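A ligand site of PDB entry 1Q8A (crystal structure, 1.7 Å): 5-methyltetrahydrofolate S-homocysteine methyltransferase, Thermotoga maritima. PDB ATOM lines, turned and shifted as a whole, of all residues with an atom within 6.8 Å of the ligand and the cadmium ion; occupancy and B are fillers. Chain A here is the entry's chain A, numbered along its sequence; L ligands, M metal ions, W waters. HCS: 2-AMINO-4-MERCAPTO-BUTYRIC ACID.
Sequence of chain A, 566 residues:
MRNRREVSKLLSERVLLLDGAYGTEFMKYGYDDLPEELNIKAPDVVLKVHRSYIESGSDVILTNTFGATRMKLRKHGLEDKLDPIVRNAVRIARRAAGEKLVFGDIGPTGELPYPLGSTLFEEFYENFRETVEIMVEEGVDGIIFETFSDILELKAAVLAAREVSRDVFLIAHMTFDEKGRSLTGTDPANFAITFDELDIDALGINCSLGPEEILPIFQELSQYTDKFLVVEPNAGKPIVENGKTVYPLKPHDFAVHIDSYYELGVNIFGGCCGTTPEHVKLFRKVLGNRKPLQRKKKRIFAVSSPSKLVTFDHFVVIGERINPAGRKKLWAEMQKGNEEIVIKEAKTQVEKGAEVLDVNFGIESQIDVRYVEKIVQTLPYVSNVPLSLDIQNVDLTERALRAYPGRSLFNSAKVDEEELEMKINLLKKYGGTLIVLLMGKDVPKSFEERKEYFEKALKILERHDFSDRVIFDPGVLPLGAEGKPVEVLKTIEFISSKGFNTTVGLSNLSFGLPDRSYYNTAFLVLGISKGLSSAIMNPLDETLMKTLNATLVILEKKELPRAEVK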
ATOM      1  N   ASP A  19      12.421  15.596 -21.283  1.00  0.00           N
ATOM      2  CA  ASP A  19      13.440  16.486 -21.863  1.00  0.00           C
ATOM      3  C   ASP A  19      13.046  16.929 -23.272  1.00  0.00           C
ATOM      4  O   ASP A  19      11.912  16.653 -23.722  1.00  0.00           O
ATOM      5  CB  ASP A  19      14.804  15.783 -21.857  1.00  0.00           C
ATOM      6  CG  ASP A  19      14.760  14.395 -22.518  1.00  0.00           C
ATOM      7  OD1 ASP A  19      15.755  13.678 -22.358  1.00  0.00           O
ATOM      8  OD2 ASP A  19      13.727  14.080 -23.134  1.00  0.00           O
ATOM      9  N   GLY A  20      13.972  17.624 -23.928  1.00  0.00           N
ATOM     10  CA  GLY A  20      13.712  18.087 -25.285  1.00  0.00           C
ATOM     11  C   GLY A  20      14.324  17.142 -26.315  1.00  0.00           C
ATOM     12  O   GLY A  20      14.424  15.936 -26.111  1.00  0.00           O
ATOM     13  N   ALA A  21      14.720  17.703 -27.445  1.00  0.00           N
ATOM     14  CA  ALA A  21      15.328  16.861 -28.491  1.00  0.00           C
ATOM     15  C   ALA A  21      16.814  16.673 -28.349  1.00  0.00           C
ATOM     16  O   ALA A  21      17.532  17.457 -27.702  1.00  0.00           O
ATOM     17  CB  ALA A  21      15.029  17.475 -29.901  1.00  0.00           C
ATOM     18  N   TYR A  22      17.317  15.613 -28.984  1.00  0.00           N
ATOM     19  CA  TYR A  22      18.723  15.336 -28.986  1.00  0.00           C
ATOM     20  C   TYR A  22      19.277  15.448 -30.407  1.00  0.00           C
ATOM     21  O   TYR A  22      20.262  16.132 -30.626  1.00  0.00           O
ATOM     22  CB  TYR A  22      18.987  13.929 -28.445  1.00  0.00           C
ATOM     23  CG  TYR A  22      18.800  13.900 -26.951  1.00  0.00           C
ATOM     24  CD1 TYR A  22      17.519  13.758 -26.403  1.00  0.00           C
ATOM     25  CD2 TYR A  22      19.867  14.101 -26.120  1.00  0.00           C
ATOM     26  CE1 TYR A  22      17.328  13.834 -25.024  1.00  0.00           C
ATOM     27  CE2 TYR A  22      19.692  14.177 -24.726  1.00  0.00           C
ATOM     28  CZ  TYR A  22      18.431  14.057 -24.202  1.00  0.00           C
ATOM     29  OH  TYR A  22      18.258  14.204 -22.821  1.00  0.00           O
ATOM     30  N   GLY A  23      18.622  14.752 -31.320  1.00  0.00           N
ATOM     31  CA  GLY A  23      19.066  14.738 -32.705  1.00  0.00           C
ATOM     32  C   GLY A  23      19.138  16.163 -33.234  1.00  0.00           C
ATOM     33  O   GLY A  23      20.141  16.533 -33.854  1.00  0.00           O
ATOM     34  N   THR A  24      18.112  16.980 -32.967  1.00  0.00           N
ATOM     35  CA  THR A  24      18.173  18.370 -33.443  1.00  0.00           C
ATOM     36  C   THR A  24      19.086  19.277 -32.599  1.00  0.00           C
ATOM     37  O   THR A  24      19.296  20.469 -32.952  1.00  0.00           O
ATOM     38  CB  THR A  24      16.768  19.001 -33.610  1.00  0.00           C
ATOM     39  OG1 THR A  24      16.062  18.996 -32.368  1.00  0.00           O
ATOM     40  CG2 THR A  24      15.977  18.255 -34.609  1.00  0.00           C
ATOM     41  N   PHE A  26      22.419  18.047 -31.350  1.00  0.00           N
ATOM     42  CA  PHE A  26      23.825  17.754 -31.588  1.00  0.00           C
ATOM     43  C   PHE A  26      24.527  18.614 -32.673  1.00  0.00           C
ATOM     44  O   PHE A  26      25.708  18.956 -32.508  1.00  0.00           O
ATOM     45  CB  PHE A  26      23.997  16.260 -31.909  1.00  0.00           C
ATOM     46  CG  PHE A  26      23.661  15.348 -30.736  1.00  0.00           C
ATOM     47  CD1 PHE A  26      22.843  14.230 -30.930  1.00  0.00           C
ATOM     48  CD2 PHE A  26      24.215  15.569 -29.485  1.00  0.00           C
ATOM     49  CE1 PHE A  26      22.596  13.356 -29.888  1.00  0.00           C
ATOM     50  CE2 PHE A  26      23.971  14.691 -28.418  1.00  0.00           C
ATOM     51  CZ  PHE A  26      23.153  13.573 -28.646  1.00  0.00           C
ATOM     52  N   PRO A  35      23.380  10.254 -34.274  1.00  0.00           N
ATOM     53  CA  PRO A  35      23.376  10.454 -32.809  1.00  0.00           C
ATOM     54  C   PRO A  35      23.933   9.285 -31.975  1.00  0.00           C
ATOM     55  O   PRO A  35      24.716   9.501 -31.043  1.00  0.00           O
ATOM     56  CB  PRO A  35      21.900  10.674 -32.510  1.00  0.00           C
ATOM     57  CG  PRO A  35      21.411  11.448 -33.734  1.00  0.00           C
ATOM     58  CD  PRO A  35      22.082  10.630 -34.869  1.00  0.00           C
ATOM     59  N   LEU A  62      15.867  10.968 -21.584  1.00  0.00           N
ATOM     60  CA  LEU A  62      15.912   9.775 -22.454  1.00  0.00           C
ATOM     61  C   LEU A  62      17.350   9.419 -22.847  1.00  0.00           C
ATOM     62  O   LEU A  62      18.143  10.311 -23.150  1.00  0.00           O
ATOM     63  CB  LEU A  62      15.164  10.089 -23.763  1.00  0.00           C
ATOM     64  CG  LEU A  62      13.700  10.503 -23.628  1.00  0.00           C
ATOM     65  CD1 LEU A  62      13.128  10.699 -25.032  1.00  0.00           C
ATOM     66  CD2 LEU A  62      12.930   9.431 -22.838  1.00  0.00           C
ATOM     67  N   THR A  63      17.668   8.126 -22.925  1.00  0.00           N
ATOM     68  CA  THR A  63      19.010   7.720 -23.338  1.00  0.00           C
ATOM     69  C   THR A  63      19.120   7.991 -24.863  1.00  0.00           C
ATOM     70  O   THR A  63      18.097   7.954 -25.575  1.00  0.00           O
ATOM     71  CB  THR A  63      19.271   6.218 -23.083  1.00  0.00           C
ATOM     72  OG1 THR A  63      18.256   5.421 -23.699  1.00  0.00           O
ATOM     73  CG2 THR A  63      19.269   5.933 -21.567  1.00  0.00           C
ATOM     74  N   ASN A  64      20.341   8.187 -25.304  1.00  0.00           N
ATOM     75  CA  ASN A  64      20.660   8.514 -26.703  1.00  0.00           C
ATOM     76  C   ASN A  64      20.746   7.227 -27.506  1.00  0.00           C
ATOM     77  O   ASN A  64      21.803   6.872 -28.094  1.00  0.00           O
ATOM     78  CB  ASN A  64      21.956   9.294 -26.738  1.00  0.00           C
ATOM     79  CG  ASN A  64      22.339   9.713 -28.140  1.00  0.00           C
ATOM     80  OD1 ASN A  64      21.463  10.019 -28.921  1.00  0.00           O
ATOM     81  ND2 ASN A  64      23.618   9.740 -28.428  1.00  0.00           N
ATOM     82  N   PHE A  66      17.800   6.191 -29.664  1.00  0.00           N
ATOM     83  CA  PHE A  66      16.659   6.117 -30.549  1.00  0.00           C
ATOM     84  C   PHE A  66      16.848   5.145 -31.721  1.00  0.00           C
ATOM     85  O   PHE A  66      15.960   4.368 -32.000  1.00  0.00           O
ATOM     86  CB  PHE A  66      16.321   7.529 -31.090  1.00  0.00           C
ATOM     87  CG  PHE A  66      15.123   7.547 -31.959  1.00  0.00           C
ATOM     88  CD1 PHE A  66      15.265   7.636 -33.355  1.00  0.00           C
ATOM     89  CD2 PHE A  66      13.851   7.479 -31.445  1.00  0.00           C
ATOM     90  CE1 PHE A  66      14.135   7.642 -34.178  1.00  0.00           C
ATOM     91  CE2 PHE A  66      12.686   7.485 -32.257  1.00  0.00           C
ATOM     92  CZ  PHE A  66      12.828   7.561 -33.626  1.00  0.00           C
ATOM     93  N   ASP A 105      15.415   4.750 -24.475  1.00  0.00           N
ATOM     94  CA  ASP A 105      14.649   5.253 -25.625  1.00  0.00           C
ATOM     95  C   ASP A 105      14.845   4.346 -26.862  1.00  0.00           C
ATOM     96  O   ASP A 105      15.945   4.106 -27.281  1.00  0.00           O
ATOM     97  CB  ASP A 105      15.177   6.679 -25.896  1.00  0.00           C
ATOM     98  CG  ASP A 105      14.480   7.387 -27.023  1.00  0.00           C
ATOM     99  OD1 ASP A 105      13.255   7.204 -27.224  1.00  0.00           O
ATOM    100  OD2 ASP A 105      15.188   8.180 -27.720  1.00  0.00           O
ATOM    101  N   GLU A 146       9.453   5.317 -28.803  1.00  0.00           N
ATOM    102  CA  GLU A 146       9.047   6.608 -29.408  1.00  0.00           C
ATOM    103  C   GLU A 146       8.869   6.588 -30.899  1.00  0.00           C
ATOM    104  O   GLU A 146       9.544   5.821 -31.569  1.00  0.00           O
ATOM    105  CB  GLU A 146      10.138   7.651 -29.166  1.00  0.00           C
ATOM    106  CG  GLU A 146      10.118   8.431 -27.802  1.00  0.00           C
ATOM    107  CD  GLU A 146      11.167   9.526 -27.809  1.00  0.00           C
ATOM    108  OE1 GLU A 146      10.803  10.693 -27.469  1.00  0.00           O
ATOM    109  OE2 GLU A 146      12.333   9.230 -28.157  1.00  0.00           O
ATOM    110  N   THR A 147       7.940   7.404 -31.394  1.00  0.00           N
ATOM    111  CA  THR A 147       7.850   7.622 -32.846  1.00  0.00           C
ATOM    112  C   THR A 147       7.488   6.399 -33.677  1.00  0.00           C
ATOM    113  O   THR A 147       7.901   6.301 -34.865  1.00  0.00           O
ATOM    114  CB  THR A 147       9.212   8.192 -33.326  1.00  0.00           C
ATOM    115  OG1 THR A 147       9.804   9.019 -32.335  1.00  0.00           O
ATOM    116  CG2 THR A 147       9.039   9.084 -34.569  1.00  0.00           C
ATOM    117  N   ASN A 206       4.381  11.426 -29.878  1.00  0.00           N
ATOM    118  CA  ASN A 206       5.500  12.344 -30.000  1.00  0.00           C
ATOM    119  C   ASN A 206       5.762  12.511 -31.479  1.00  0.00           C
ATOM    120  O   ASN A 206       5.314  11.660 -32.268  1.00  0.00           O
ATOM    121  CB  ASN A 206       6.812  11.898 -29.310  1.00  0.00           C
ATOM    122  CG  ASN A 206       7.461  10.674 -30.000  1.00  0.00           C
ATOM    123  OD1 ASN A 206       6.945   9.562 -29.882  1.00  0.00           O
ATOM    124  ND2 ASN A 206       8.572  10.911 -30.706  1.00  0.00           N
ATOM    125  N   CYS A 207       6.368  13.662 -31.795  1.00  0.00           N
ATOM    126  CA  CYS A 207       6.827  14.011 -33.129  1.00  0.00           C
ATOM    127  C   CYS A 207       5.743  14.310 -34.153  1.00  0.00           C
ATOM    128  O   CYS A 207       4.531  14.298 -33.873  1.00  0.00           O
ATOM    129  CB  CYS A 207       7.783  12.911 -33.645  1.00  0.00           C
ATOM    130  SG  CYS A 207       9.022  13.400 -34.920  1.00  0.00           S
ATOM    131  N   SER A 208       6.233  14.551 -35.363  1.00  0.00           N
ATOM    132  CA  SER A 208       5.441  14.851 -36.536  1.00  0.00           C
ATOM    133  C   SER A 208       4.711  16.184 -36.544  1.00  0.00           C
ATOM    134  O   SER A 208       4.632  16.832 -37.576  1.00  0.00           O
ATOM    135  CB  SER A 208       4.398  13.755 -36.813  1.00  0.00           C
ATOM    136  OG  SER A 208       5.026  12.552 -37.230  1.00  0.00           O
ATOM    137  N   GLU A 232       5.002  14.471 -26.330  1.00  0.00           N
ATOM    138  CA  GLU A 232       6.206  15.208 -26.682  1.00  0.00           C
ATOM    139  C   GLU A 232       6.049  15.782 -28.093  1.00  0.00           C
ATOM    140  O   GLU A 232       6.574  15.221 -29.075  1.00  0.00           O
ATOM    141  CB  GLU A 232       7.498  14.352 -26.675  1.00  0.00           C
ATOM    142  CG  GLU A 232       7.853  13.676 -25.359  1.00  0.00           C
ATOM    143  CD  GLU A 232       8.969  12.673 -25.613  1.00  0.00           C
ATOM    144  OE1 GLU A 232      10.128  12.943 -25.274  1.00  0.00           O
ATOM    145  OE2 GLU A 232       8.640  11.639 -26.215  1.00  0.00           O
ATOM    146  N   ASN A 234       6.582  18.190 -31.443  1.00  0.00           N
ATOM    147  CA  ASN A 234       7.715  18.885 -31.987  1.00  0.00           C
ATOM    148  C   ASN A 234       7.399  20.371 -31.615  1.00  0.00           C
ATOM    149  O   ASN A 234       6.254  20.688 -31.291  1.00  0.00           O
ATOM    150  CB  ASN A 234       7.711  18.879 -33.523  1.00  0.00           C
ATOM    151  CG  ASN A 234       8.114  17.557 -34.071  1.00  0.00           C
ATOM    152  OD1 ASN A 234       8.823  16.786 -33.401  1.00  0.00           O
ATOM    153  ND2 ASN A 234       7.731  17.292 -35.313  1.00  0.00           N
ATOM    154  N   TYR A 247      12.085  24.133 -36.841  1.00  0.00           N
ATOM    155  CA  TYR A 247      10.939  23.988 -35.958  1.00  0.00           C
ATOM    156  C   TYR A 247      10.832  25.407 -35.372  1.00  0.00           C
ATOM    157  O   TYR A 247      11.593  25.800 -34.508  1.00  0.00           O
ATOM    158  CB  TYR A 247      11.259  22.922 -34.908  1.00  0.00           C
ATOM    159  CG  TYR A 247      11.391  21.529 -35.529  1.00  0.00           C
ATOM    160  CD1 TYR A 247      10.261  20.771 -35.807  1.00  0.00           C
ATOM    161  CD2 TYR A 247      12.646  21.013 -35.873  1.00  0.00           C
ATOM    162  CE1 TYR A 247      10.377  19.498 -36.431  1.00  0.00           C
ATOM    163  CE2 TYR A 247      12.764  19.749 -36.500  1.00  0.00           C
ATOM    164  CZ  TYR A 247      11.612  19.009 -36.768  1.00  0.00           C
ATOM    165  OH  TYR A 247      11.712  17.770 -37.398  1.00  0.00           O
ATOM    166  N   GLY A 271       9.214  17.499 -24.985  1.00  0.00           N
ATOM    167  CA  GLY A 271       9.194  17.921 -26.381  1.00  0.00           C
ATOM    168  C   GLY A 271      10.046  17.000 -27.231  1.00  0.00           C
ATOM    169  O   GLY A 271      10.960  16.324 -26.702  1.00  0.00           O
ATOM    170  N   CYS A 272       9.756  16.971 -28.542  1.00  0.00           N
ATOM    171  CA  CYS A 272      10.528  16.141 -29.502  1.00  0.00           C
ATOM    172  C   CYS A 272      11.353  17.092 -30.410  1.00  0.00           C
ATOM    173  O   CYS A 272      11.712  18.223 -29.997  1.00  0.00           O
ATOM    174  CB  CYS A 272       9.578  15.272 -30.315  1.00  0.00           C
ATOM    175  SG  CYS A 272      10.514  13.735 -30.956  1.00  0.00           S
ATOM    176  N   CYS A 273      11.653  16.657 -31.631  1.00  0.00           N
ATOM    177  CA  CYS A 273      12.449  17.442 -32.543  1.00  0.00           C
ATOM    178  C   CYS A 273      12.100  18.924 -32.497  1.00  0.00           C
ATOM    179  O   CYS A 273      10.931  19.296 -32.506  1.00  0.00           O
ATOM    180  CB  CYS A 273      12.261  16.903 -33.962  1.00  0.00           C
ATOM    181  SG  CYS A 273      12.928  15.179 -34.097  1.00  0.00           S
ATOM    182  N   GLY A 274      13.149  19.740 -32.405  1.00  0.00           N
ATOM    183  CA  GLY A 274      13.011  21.183 -32.374  1.00  0.00           C
ATOM    184  C   GLY A 274      12.967  21.802 -30.993  1.00  0.00           C
ATOM    185  O   GLY A 274      13.207  23.010 -30.839  1.00  0.00           O
HETATM  186  N   HCS L   1      14.387  11.114 -28.701  1.00  0.00           N
HETATM  187  CA  HCS L   1      14.723  11.310 -30.136  1.00  0.00           C
HETATM  188  CB  HCS L   1      13.399  11.330 -30.942  1.00  0.00           C
HETATM  189  CG  HCS L   1      13.622  11.252 -32.487  1.00  0.00           C
HETATM  190  SD  HCS L   1      12.088  11.181 -33.428  1.00  0.00           S
HETATM  191  C   HCS L   1      15.520  12.649 -30.289  1.00  0.00           C
HETATM  192  OXT HCS L   1      16.295  12.767 -31.278  1.00  0.00           O
HETATM  193  O   HCS L   1      15.328  13.514 -29.410  1.00  0.00           O
HETATM  194 CD    CD M   1      11.116  13.494 -33.248  1.00  0.00          CD
HETATM  195  O   HOH W   1      15.833  15.181 -32.549  1.00  0.00           O
HETATM  196  O   HOH W   2      18.121  10.595 -31.993  1.00  0.00           O
HETATM  197  O   HOH W   3      12.324  12.931 -27.772  1.00  0.00           O
HETATM  198  O   HOH W   4      16.882  10.228 -27.677  1.00  0.00           O
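A sulfur (SD) of the ligand lies close to the side-chain hydroxyl (OG1) of Thr 147.
OXT of the ligand is in hydrogen-bond range of N of Gly 23 (3.1 Å).
OE2 of Glu 146 is in salt-bridge range of N of the ligand.
OD2 of Asp 105 lies within salt-bridge range of N of the ligand (3.2 Å).
The backbone NH of Tyr 22 is in hydrogen-bond range of an oxygen (O) of the ligand (2.9 Å).
Three residues have an atom within 4 Å of the cadmium ion: Cys 207, Cys 272 and Cys 273.
The side-chain sulfur of Cys 272 sits close to the side-chain amide nitrogen of Asn 206 (3.4 Å).
OH of Tyr 22 lies within hydrogen-bond range of OD1 of Asp 19 (2.6 Å).
OE2 of Glu 146 sits close to OD1 of Asp 105 (2.4 Å).
The backbone NH of Cys 273 sits at hydrogen-bond distance from the side-chain amide oxygen of Asn 234, at 3.3 Å.
N of Asp 105 sits at hydrogen-bond distance from OG1 of Thr 63, at 3.0 Å.
SG of Cys 207 lies close to OD1 of Asn 234, at 3.7 Å.
N of Cys 207 sits at hydrogen-bond distance from O of Glu 232.
The side-chain hydroxyl of Thr 147 sits at hydrogen-bond distance from the side-chain amide nitrogen of Asn 206, at 2.8 Å.
The cadmium ion is bound by the side-chain sulfur (SG) of Cys 272 (2.4 Å), a sulfur (SD) of the ligand (2.5 Å), the side-chain sulfur (SG) of Cys 273 (2.6 Å) and the side-chain sulfur (SG) of Cys 207 (2.7 Å).
The cadmium ion has four donor atoms within binding distance.
Ala 21 touches the ligand.
Leu 62 touches the ligand (CD1 to N, 3.9 Å).
CZ of Phe 66 touches SD of the ligand (3.7 Å).
Hydrophobic or aromatic side chains within 4 Å of the ligand: Tyr 22, Leu 62 and Phe 66.
The nearest printed residue that does not touch the ligand is Cys 207 (4.1 Å).
Water W1 lies within hydrogen-bond range of OXT of the ligand, N of Thr 24 and N of Gly 23.
Water W4 lies within hydrogen-bond range of OD2 of Asp 105, N of the ligand and O of Thr 63.
Water W3 lies within hydrogen-bond range of OE1 of Glu 146, N of the ligand and OE1 of Glu 232.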
